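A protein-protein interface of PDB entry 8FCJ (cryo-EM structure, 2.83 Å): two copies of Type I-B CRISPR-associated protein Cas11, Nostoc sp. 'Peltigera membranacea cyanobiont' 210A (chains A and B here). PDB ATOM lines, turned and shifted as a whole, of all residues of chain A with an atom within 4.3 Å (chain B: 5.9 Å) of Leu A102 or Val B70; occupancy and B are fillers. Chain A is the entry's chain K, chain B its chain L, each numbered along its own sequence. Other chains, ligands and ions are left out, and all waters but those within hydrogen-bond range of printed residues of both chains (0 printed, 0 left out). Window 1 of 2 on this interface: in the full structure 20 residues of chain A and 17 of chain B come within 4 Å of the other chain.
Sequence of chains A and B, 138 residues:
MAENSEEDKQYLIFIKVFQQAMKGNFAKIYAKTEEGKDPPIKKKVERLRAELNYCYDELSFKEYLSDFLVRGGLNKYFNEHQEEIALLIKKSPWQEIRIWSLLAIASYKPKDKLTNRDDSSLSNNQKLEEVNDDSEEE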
ATOM      1  N   ARG A  49      26.572  20.759  -1.983  1.00  0.00           N
ATOM      2  CA  ARG A  49      25.629  20.394  -3.036  1.00  0.00           C
ATOM      3  C   ARG A  49      24.443  21.349  -3.078  1.00  0.00           C
ATOM      4  O   ARG A  49      24.040  21.815  -4.152  1.00  0.00           O
ATOM      5  CB  ARG A  49      25.154  18.958  -2.815  1.00  0.00           C
ATOM      6  CG  ARG A  49      24.560  18.275  -4.026  1.00  0.00           C
ATOM      7  CD  ARG A  49      23.084  18.559  -4.142  1.00  0.00           C
ATOM      8  NE  ARG A  49      22.297  17.728  -3.241  1.00  0.00           N
ATOM      9  CZ  ARG A  49      20.976  17.768  -3.152  1.00  0.00           C
ATOM     10  NH1 ARG A  49      20.254  18.568  -3.919  1.00  0.00           N
ATOM     11  NH2 ARG A  49      20.362  16.989  -2.266  1.00  0.00           N
ATOM     12  N   LEU A  52      25.418  24.581  -4.491  1.00  0.00           N
ATOM     13  CA  LEU A  52      25.653  24.485  -5.928  1.00  0.00           C
ATOM     14  C   LEU A  52      24.343  24.511  -6.705  1.00  0.00           C
ATOM     15  O   LEU A  52      24.222  25.224  -7.707  1.00  0.00           O
ATOM     16  CB  LEU A  52      26.449  23.222  -6.248  1.00  0.00           C
ATOM     17  CG  LEU A  52      27.970  23.342  -6.150  1.00  0.00           C
ATOM     18  CD1 LEU A  52      28.643  22.120  -6.744  1.00  0.00           C
ATOM     19  CD2 LEU A  52      28.453  24.602  -6.842  1.00  0.00           C
ATOM     20  N   ARG A  98      28.853  23.579 -13.635  1.00  0.00           N
ATOM     21  CA  ARG A  98      28.218  22.988 -12.460  1.00  0.00           C
ATOM     22  C   ARG A  98      28.261  21.469 -12.517  1.00  0.00           C
ATOM     23  O   ARG A  98      28.474  20.806 -11.496  1.00  0.00           O
ATOM     24  CB  ARG A  98      26.776  23.475 -12.334  1.00  0.00           C
ATOM     25  CG  ARG A  98      26.117  23.076 -11.025  1.00  0.00           C
ATOM     26  CD  ARG A  98      24.882  23.909 -10.742  1.00  0.00           C
ATOM     27  NE  ARG A  98      23.823  23.662 -11.711  1.00  0.00           N
ATOM     28  CZ  ARG A  98      22.619  24.214 -11.661  1.00  0.00           C
ATOM     29  NH1 ARG A  98      22.286  25.056 -10.698  1.00  0.00           N
ATOM     30  NH2 ARG A  98      21.727  23.912 -12.599  1.00  0.00           N
ATOM     31  N   ILE A  99      28.049  20.898 -13.703  1.00  0.00           N
ATOM     32  CA  ILE A  99      28.157  19.450 -13.859  1.00  0.00           C
ATOM     33  C   ILE A  99      29.569  18.987 -13.522  1.00  0.00           C
ATOM     34  O   ILE A  99      29.761  17.987 -12.816  1.00  0.00           O
ATOM     35  CB  ILE A  99      27.751  19.031 -15.283  1.00  0.00           C
ATOM     36  CG1 ILE A  99      26.246  19.207 -15.483  1.00  0.00           C
ATOM     37  CG2 ILE A  99      28.154  17.596 -15.554  1.00  0.00           C
ATOM     38  CD1 ILE A  99      25.860  19.534 -16.903  1.00  0.00           C
ATOM     39  N   TRP A 100      30.575  19.709 -14.015  1.00  0.00           N
ATOM     40  CA  TRP A 100      31.960  19.354 -13.710  1.00  0.00           C
ATOM     41  C   TRP A 100      32.243  19.466 -12.217  1.00  0.00           C
ATOM     42  O   TRP A 100      32.943  18.625 -11.644  1.00  0.00           O
ATOM     43  CB  TRP A 100      32.922  20.244 -14.494  1.00  0.00           C
ATOM     44  CG  TRP A 100      32.704  20.231 -15.965  1.00  0.00           C
ATOM     45  CD1 TRP A 100      32.036  19.291 -16.688  1.00  0.00           C
ATOM     46  CD2 TRP A 100      33.162  21.209 -16.902  1.00  0.00           C
ATOM     47  NE1 TRP A 100      32.047  19.624 -18.019  1.00  0.00           N
ATOM     48  CE2 TRP A 100      32.732  20.798 -18.176  1.00  0.00           C
ATOM     49  CE3 TRP A 100      33.892  22.394 -16.785  1.00  0.00           C
ATOM     50  CZ2 TRP A 100      33.008  21.529 -19.325  1.00  0.00           C
ATOM     51  CZ3 TRP A 100      34.165  23.117 -17.925  1.00  0.00           C
ATOM     52  CH2 TRP A 100      33.725  22.683 -19.180  1.00  0.00           C
ATOM     53  N   SER A 101      31.719  20.511 -11.574  1.00  0.00           N
ATOM     54  CA  SER A 101      31.925  20.687 -10.142  1.00  0.00           C
ATOM     55  C   SER A 101      31.293  19.552  -9.352  1.00  0.00           C
ATOM     56  O   SER A 101      31.890  19.042  -8.400  1.00  0.00           O
ATOM     57  CB  SER A 101      31.359  22.032  -9.694  1.00  0.00           C
ATOM     58  OG  SER A 101      31.544  23.016 -10.695  1.00  0.00           O
ATOM     59  N   LEU A 102      30.083  19.142  -9.731  1.00  0.00           N
ATOM     60  CA  LEU A 102      29.444  18.021  -9.051  1.00  0.00           C
ATOM     61  C   LEU A 102      30.223  16.730  -9.271  1.00  0.00           C
ATOM     62  O   LEU A 102      30.378  15.924  -8.345  1.00  0.00           O
ATOM     63  CB  LEU A 102      28.001  17.872  -9.526  1.00  0.00           C
ATOM     64  CG  LEU A 102      27.049  18.994  -9.113  1.00  0.00           C
ATOM     65  CD1 LEU A 102      25.857  19.058 -10.047  1.00  0.00           C
ATOM     66  CD2 LEU A 102      26.597  18.809  -7.677  1.00  0.00           C
ATOM     67  N   LEU A 103      30.732  16.519 -10.486  1.00  0.00           N
ATOM     68  CA  LEU A 103      31.542  15.333 -10.740  1.00  0.00           C
ATOM     69  C   LEU A 103      32.805  15.342  -9.889  1.00  0.00           C
ATOM     70  O   LEU A 103      33.239  14.295  -9.395  1.00  0.00           O
ATOM     71  CB  LEU A 103      31.889  15.243 -12.223  1.00  0.00           C
ATOM     72  CG  LEU A 103      30.736  14.832 -13.137  1.00  0.00           C
ATOM     73  CD1 LEU A 103      31.178  14.834 -14.588  1.00  0.00           C
ATOM     74  CD2 LEU A 103      30.204  13.468 -12.740  1.00  0.00           C
ATOM     75  N   ALA A 104      33.412  16.516  -9.713  1.00  0.00           N
ATOM     76  CA  ALA A 104      34.562  16.630  -8.821  1.00  0.00           C
ATOM     77  C   ALA A 104      34.170  16.337  -7.378  1.00  0.00           C
ATOM     78  O   ALA A 104      34.937  15.715  -6.636  1.00  0.00           O
ATOM     79  CB  ALA A 104      35.179  18.021  -8.936  1.00  0.00           C
ATOM     80  N   ILE A 105      32.987  16.791  -6.965  1.00  0.00           N
ATOM     81  CA  ILE A 105      32.514  16.534  -5.606  1.00  0.00           C
ATOM     82  C   ILE A 105      32.377  15.038  -5.370  1.00  0.00           C
ATOM     83  O   ILE A 105      32.813  14.507  -4.341  1.00  0.00           O
ATOM     84  CB  ILE A 105      31.176  17.253  -5.359  1.00  0.00           C
ATOM     85  CG1 ILE A 105      31.368  18.766  -5.316  1.00  0.00           C
ATOM     86  CG2 ILE A 105      30.557  16.765  -4.058  1.00  0.00           C
ATOM     87  CD1 ILE A 105      30.284  19.490  -4.569  1.00  0.00           C
ATOM     88  N   ALA A 106      31.773  14.333  -6.326  1.00  0.00           N
ATOM     89  CA  ALA A 106      31.502  12.911  -6.150  1.00  0.00           C
ATOM     90  C   ALA A 106      32.769  12.068  -6.112  1.00  0.00           C
ATOM     91  O   ALA A 106      32.710  10.907  -5.699  1.00  0.00           O
ATOM     92  CB  ALA A 106      30.580  12.411  -7.262  1.00  0.00           C
ATOM     93  N   LYS B  28      19.567   7.365   2.571  1.00  0.00           N
ATOM     94  CA  LYS B  28      19.096   8.675   3.006  1.00  0.00           C
ATOM     95  C   LYS B  28      17.578   8.696   3.130  1.00  0.00           C
ATOM     96  O   LYS B  28      17.033   9.223   4.108  1.00  0.00           O
ATOM     97  CB  LYS B  28      19.562   9.755   2.030  1.00  0.00           C
ATOM     98  CG  LYS B  28      21.042  10.087   2.114  1.00  0.00           C
ATOM     99  CD  LYS B  28      21.448  11.037   0.999  1.00  0.00           C
ATOM    100  CE  LYS B  28      22.351  12.145   1.514  1.00  0.00           C
ATOM    101  NZ  LYS B  28      23.726  11.653   1.802  1.00  0.00           N
ATOM    102  N   GLU B  63      23.266  16.791 -15.789  1.00  0.00           N
ATOM    103  CA  GLU B  63      23.049  17.509 -14.540  1.00  0.00           C
ATOM    104  C   GLU B  63      22.383  16.611 -13.506  1.00  0.00           C
ATOM    105  O   GLU B  63      22.820  16.541 -12.349  1.00  0.00           O
ATOM    106  CB  GLU B  63      22.201  18.754 -14.799  1.00  0.00           C
ATOM    107  CG  GLU B  63      22.404  19.872 -13.796  1.00  0.00           C
ATOM    108  CD  GLU B  63      22.110  21.236 -14.388  1.00  0.00           C
ATOM    109  OE1 GLU B  63      21.127  21.354 -15.148  1.00  0.00           O
ATOM    110  OE2 GLU B  63      22.861  22.189 -14.091  1.00  0.00           O
ATOM    111  N   LEU B  65      22.372  13.327 -13.441  1.00  0.00           N
ATOM    112  CA  LEU B  65      23.272  12.239 -13.079  1.00  0.00           C
ATOM    113  C   LEU B  65      24.328  12.702 -12.088  1.00  0.00           C
ATOM    114  O   LEU B  65      24.625  12.000 -11.116  1.00  0.00           O
ATOM    115  CB  LEU B  65      23.929  11.665 -14.331  1.00  0.00           C
ATOM    116  CG  LEU B  65      25.030  10.636 -14.083  1.00  0.00           C
ATOM    117  CD1 LEU B  65      24.435   9.333 -13.590  1.00  0.00           C
ATOM    118  CD2 LEU B  65      25.842  10.415 -15.342  1.00  0.00           C
ATOM    119  N   SER B  66      24.910  13.881 -12.316  1.00  0.00           N
ATOM    120  CA  SER B  66      25.899  14.405 -11.382  1.00  0.00           C
ATOM    121  C   SER B  66      25.278  14.676 -10.019  1.00  0.00           C
ATOM    122  O   SER B  66      25.874  14.356  -8.981  1.00  0.00           O
ATOM    123  CB  SER B  66      26.529  15.674 -11.949  1.00  0.00           C
ATOM    124  OG  SER B  66      26.657  15.588 -13.356  1.00  0.00           O
ATOM    125  N   ASP B  67      24.078  15.260 -10.000  1.00  0.00           N
ATOM    126  CA  ASP B  67      23.406  15.526  -8.734  1.00  0.00           C
ATOM    127  C   ASP B  67      23.129  14.232  -7.977  1.00  0.00           C
ATOM    128  O   ASP B  67      23.356  14.145  -6.766  1.00  0.00           O
ATOM    129  CB  ASP B  67      22.110  16.294  -8.990  1.00  0.00           C
ATOM    130  CG  ASP B  67      21.403  16.689  -7.714  1.00  0.00           C
ATOM    131  OD1 ASP B  67      21.982  17.471  -6.933  1.00  0.00           O
ATOM    132  OD2 ASP B  67      20.269  16.220  -7.493  1.00  0.00           O
ATOM    133  N   PHE B  68      22.645  13.210  -8.685  1.00  0.00           N
ATOM    134  CA  PHE B  68      22.370  11.924  -8.056  1.00  0.00           C
ATOM    135  C   PHE B  68      23.645  11.282  -7.526  1.00  0.00           C
ATOM    136  O   PHE B  68      23.666  10.749  -6.410  1.00  0.00           O
ATOM    137  CB  PHE B  68      21.680  11.002  -9.059  1.00  0.00           C
ATOM    138  CG  PHE B  68      21.243   9.693  -8.480  1.00  0.00           C
ATOM    139  CD1 PHE B  68      20.092   9.608  -7.720  1.00  0.00           C
ATOM    140  CD2 PHE B  68      21.979   8.544  -8.703  1.00  0.00           C
ATOM    141  CE1 PHE B  68      19.686   8.405  -7.189  1.00  0.00           C
ATOM    142  CE2 PHE B  68      21.578   7.339  -8.173  1.00  0.00           C
ATOM    143  CZ  PHE B  68      20.429   7.270  -7.415  1.00  0.00           C
ATOM    144  N   LEU B  69      24.722  11.328  -8.313  1.00  0.00           N
ATOM    145  CA  LEU B  69      25.983  10.740  -7.878  1.00  0.00           C
ATOM    146  C   LEU B  69      26.498  11.425  -6.624  1.00  0.00           C
ATOM    147  O   LEU B  69      26.995  10.763  -5.706  1.00  0.00           O
ATOM    148  CB  LEU B  69      27.019  10.829  -8.997  1.00  0.00           C
ATOM    149  CG  LEU B  69      26.890   9.827 -10.142  1.00  0.00           C
ATOM    150  CD1 LEU B  69      28.084   9.933 -11.071  1.00  0.00           C
ATOM    151  CD2 LEU B  69      26.755   8.420  -9.606  1.00  0.00           C
ATOM    152  N   VAL B  70      26.392  12.753  -6.565  1.00  0.00           N
ATOM    153  CA  VAL B  70      26.849  13.463  -5.375  1.00  0.00           C
ATOM    154  C   VAL B  70      25.969  13.115  -4.182  1.00  0.00           C
ATOM    155  O   VAL B  70      26.467  12.878  -3.074  1.00  0.00           O
ATOM    156  CB  VAL B  70      26.878  14.977  -5.630  1.00  0.00           C
ATOM    157  CG1 VAL B  70      26.745  15.722  -4.327  1.00  0.00           C
ATOM    158  CG2 VAL B  70      28.146  15.361  -6.334  1.00  0.00           C
ATOM    159  N   ARG B  71      24.651  13.070  -4.387  1.00  0.00           N
ATOM    160  CA  ARG B  71      23.739  12.682  -3.318  1.00  0.00           C
ATOM    161  C   ARG B  71      23.998  11.266  -2.827  1.00  0.00           C
ATOM    162  O   ARG B  71      23.621  10.937  -1.698  1.00  0.00           O
ATOM    163  CB  ARG B  71      22.292  12.806  -3.791  1.00  0.00           C
ATOM    164  CG  ARG B  71      21.615  14.098  -3.389  1.00  0.00           C
ATOM    165  CD  ARG B  71      20.107  13.951  -3.431  1.00  0.00           C
ATOM    166  NE  ARG B  71      19.650  13.435  -4.715  1.00  0.00           N
ATOM    167  CZ  ARG B  71      18.990  14.148  -5.615  1.00  0.00           C
ATOM    168  NH1 ARG B  71      18.686  15.418  -5.404  1.00  0.00           N
ATOM    169  NH2 ARG B  71      18.624  13.574  -6.758  1.00  0.00           N
ATOM    170  N   GLY B  72      24.617  10.423  -3.653  1.00  0.00           N
ATOM    171  CA  GLY B  72      24.917   9.068  -3.218  1.00  0.00           C
ATOM    172  C   GLY B  72      25.829   9.029  -2.006  1.00  0.00           C
ATOM    173  O   GLY B  72      25.570   8.307  -1.042  1.00  0.00           O
ATOM    174  N   GLY B  73      26.904   9.809  -2.034  1.00  0.00           N
ATOM    175  CA  GLY B  73      27.812   9.840  -0.904  1.00  0.00           C
ATOM    176  C   GLY B  73      29.268   9.624  -1.263  1.00  0.00           C
ATOM    177  O   GLY B  73      29.790  10.268  -2.179  1.00  0.00           O
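OD1 of Asp B67 lies within salt-bridge range of NH1 of Arg A49 (3.6 Å). The side-chain carboxylate of Glu B63 lies within salt-bridge range of the guanidinium group of Arg A98 (2.5 Å).
The side-chain carboxylate (OD2) of Asp B67 lies within salt-bridge range of the guanidinium group (NH1) of Arg B71, 2.7 Å away.
Among the printed residues, merely in contact across the chains: Arg A49 with Val B70 (3.4 Å), Arg A49 with Arg B71 (3.3 Å), Ile A99 with Glu B63 (3.7 Å), Ile A99 with Ser B66 (3.3 Å), Leu A102 with Ser B66 (3.6 Å), Leu A102 with Val B70 (3.1 Å), Ile A105 with Val B70 (3.6 Å) and Ala A106 with Val B70 (3.8 Å).
Of the printed residues of chain B, Arg A49 touches Asp B67, Val B70 and Arg B71. Of the printed residues of chain B, Ile A99 touches Glu B63 (3.7 Å) and Ser B66 (3.3 Å). Leu A102 touches two residues of chain B. Ala A104 touches none of the printed residues of chain B. Val B70 touches just these residues of chain A: Arg A49, Leu A102, Ile A105 and Ala A106. The nearest residue of chain B that does not touch Leu A102 is Asp B67 (4.2 Å). The nearest printed residue of chain A that does not touch Ser B66 is Leu A103 (4.2 Å).
Hydrophobic or aromatic side chains of chain A that line the printed part of chain B: Ile A99, Leu A102, Ile A105 and Ala A106. Hydrophobic or aromatic side chains of chain B within 4 Å of the printed part of chain A: Val B70.
No position is printed for both chains. Of the 10 pairs that touch across the chains among the printed residues, none has its exchanged pair printed and touching as well.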
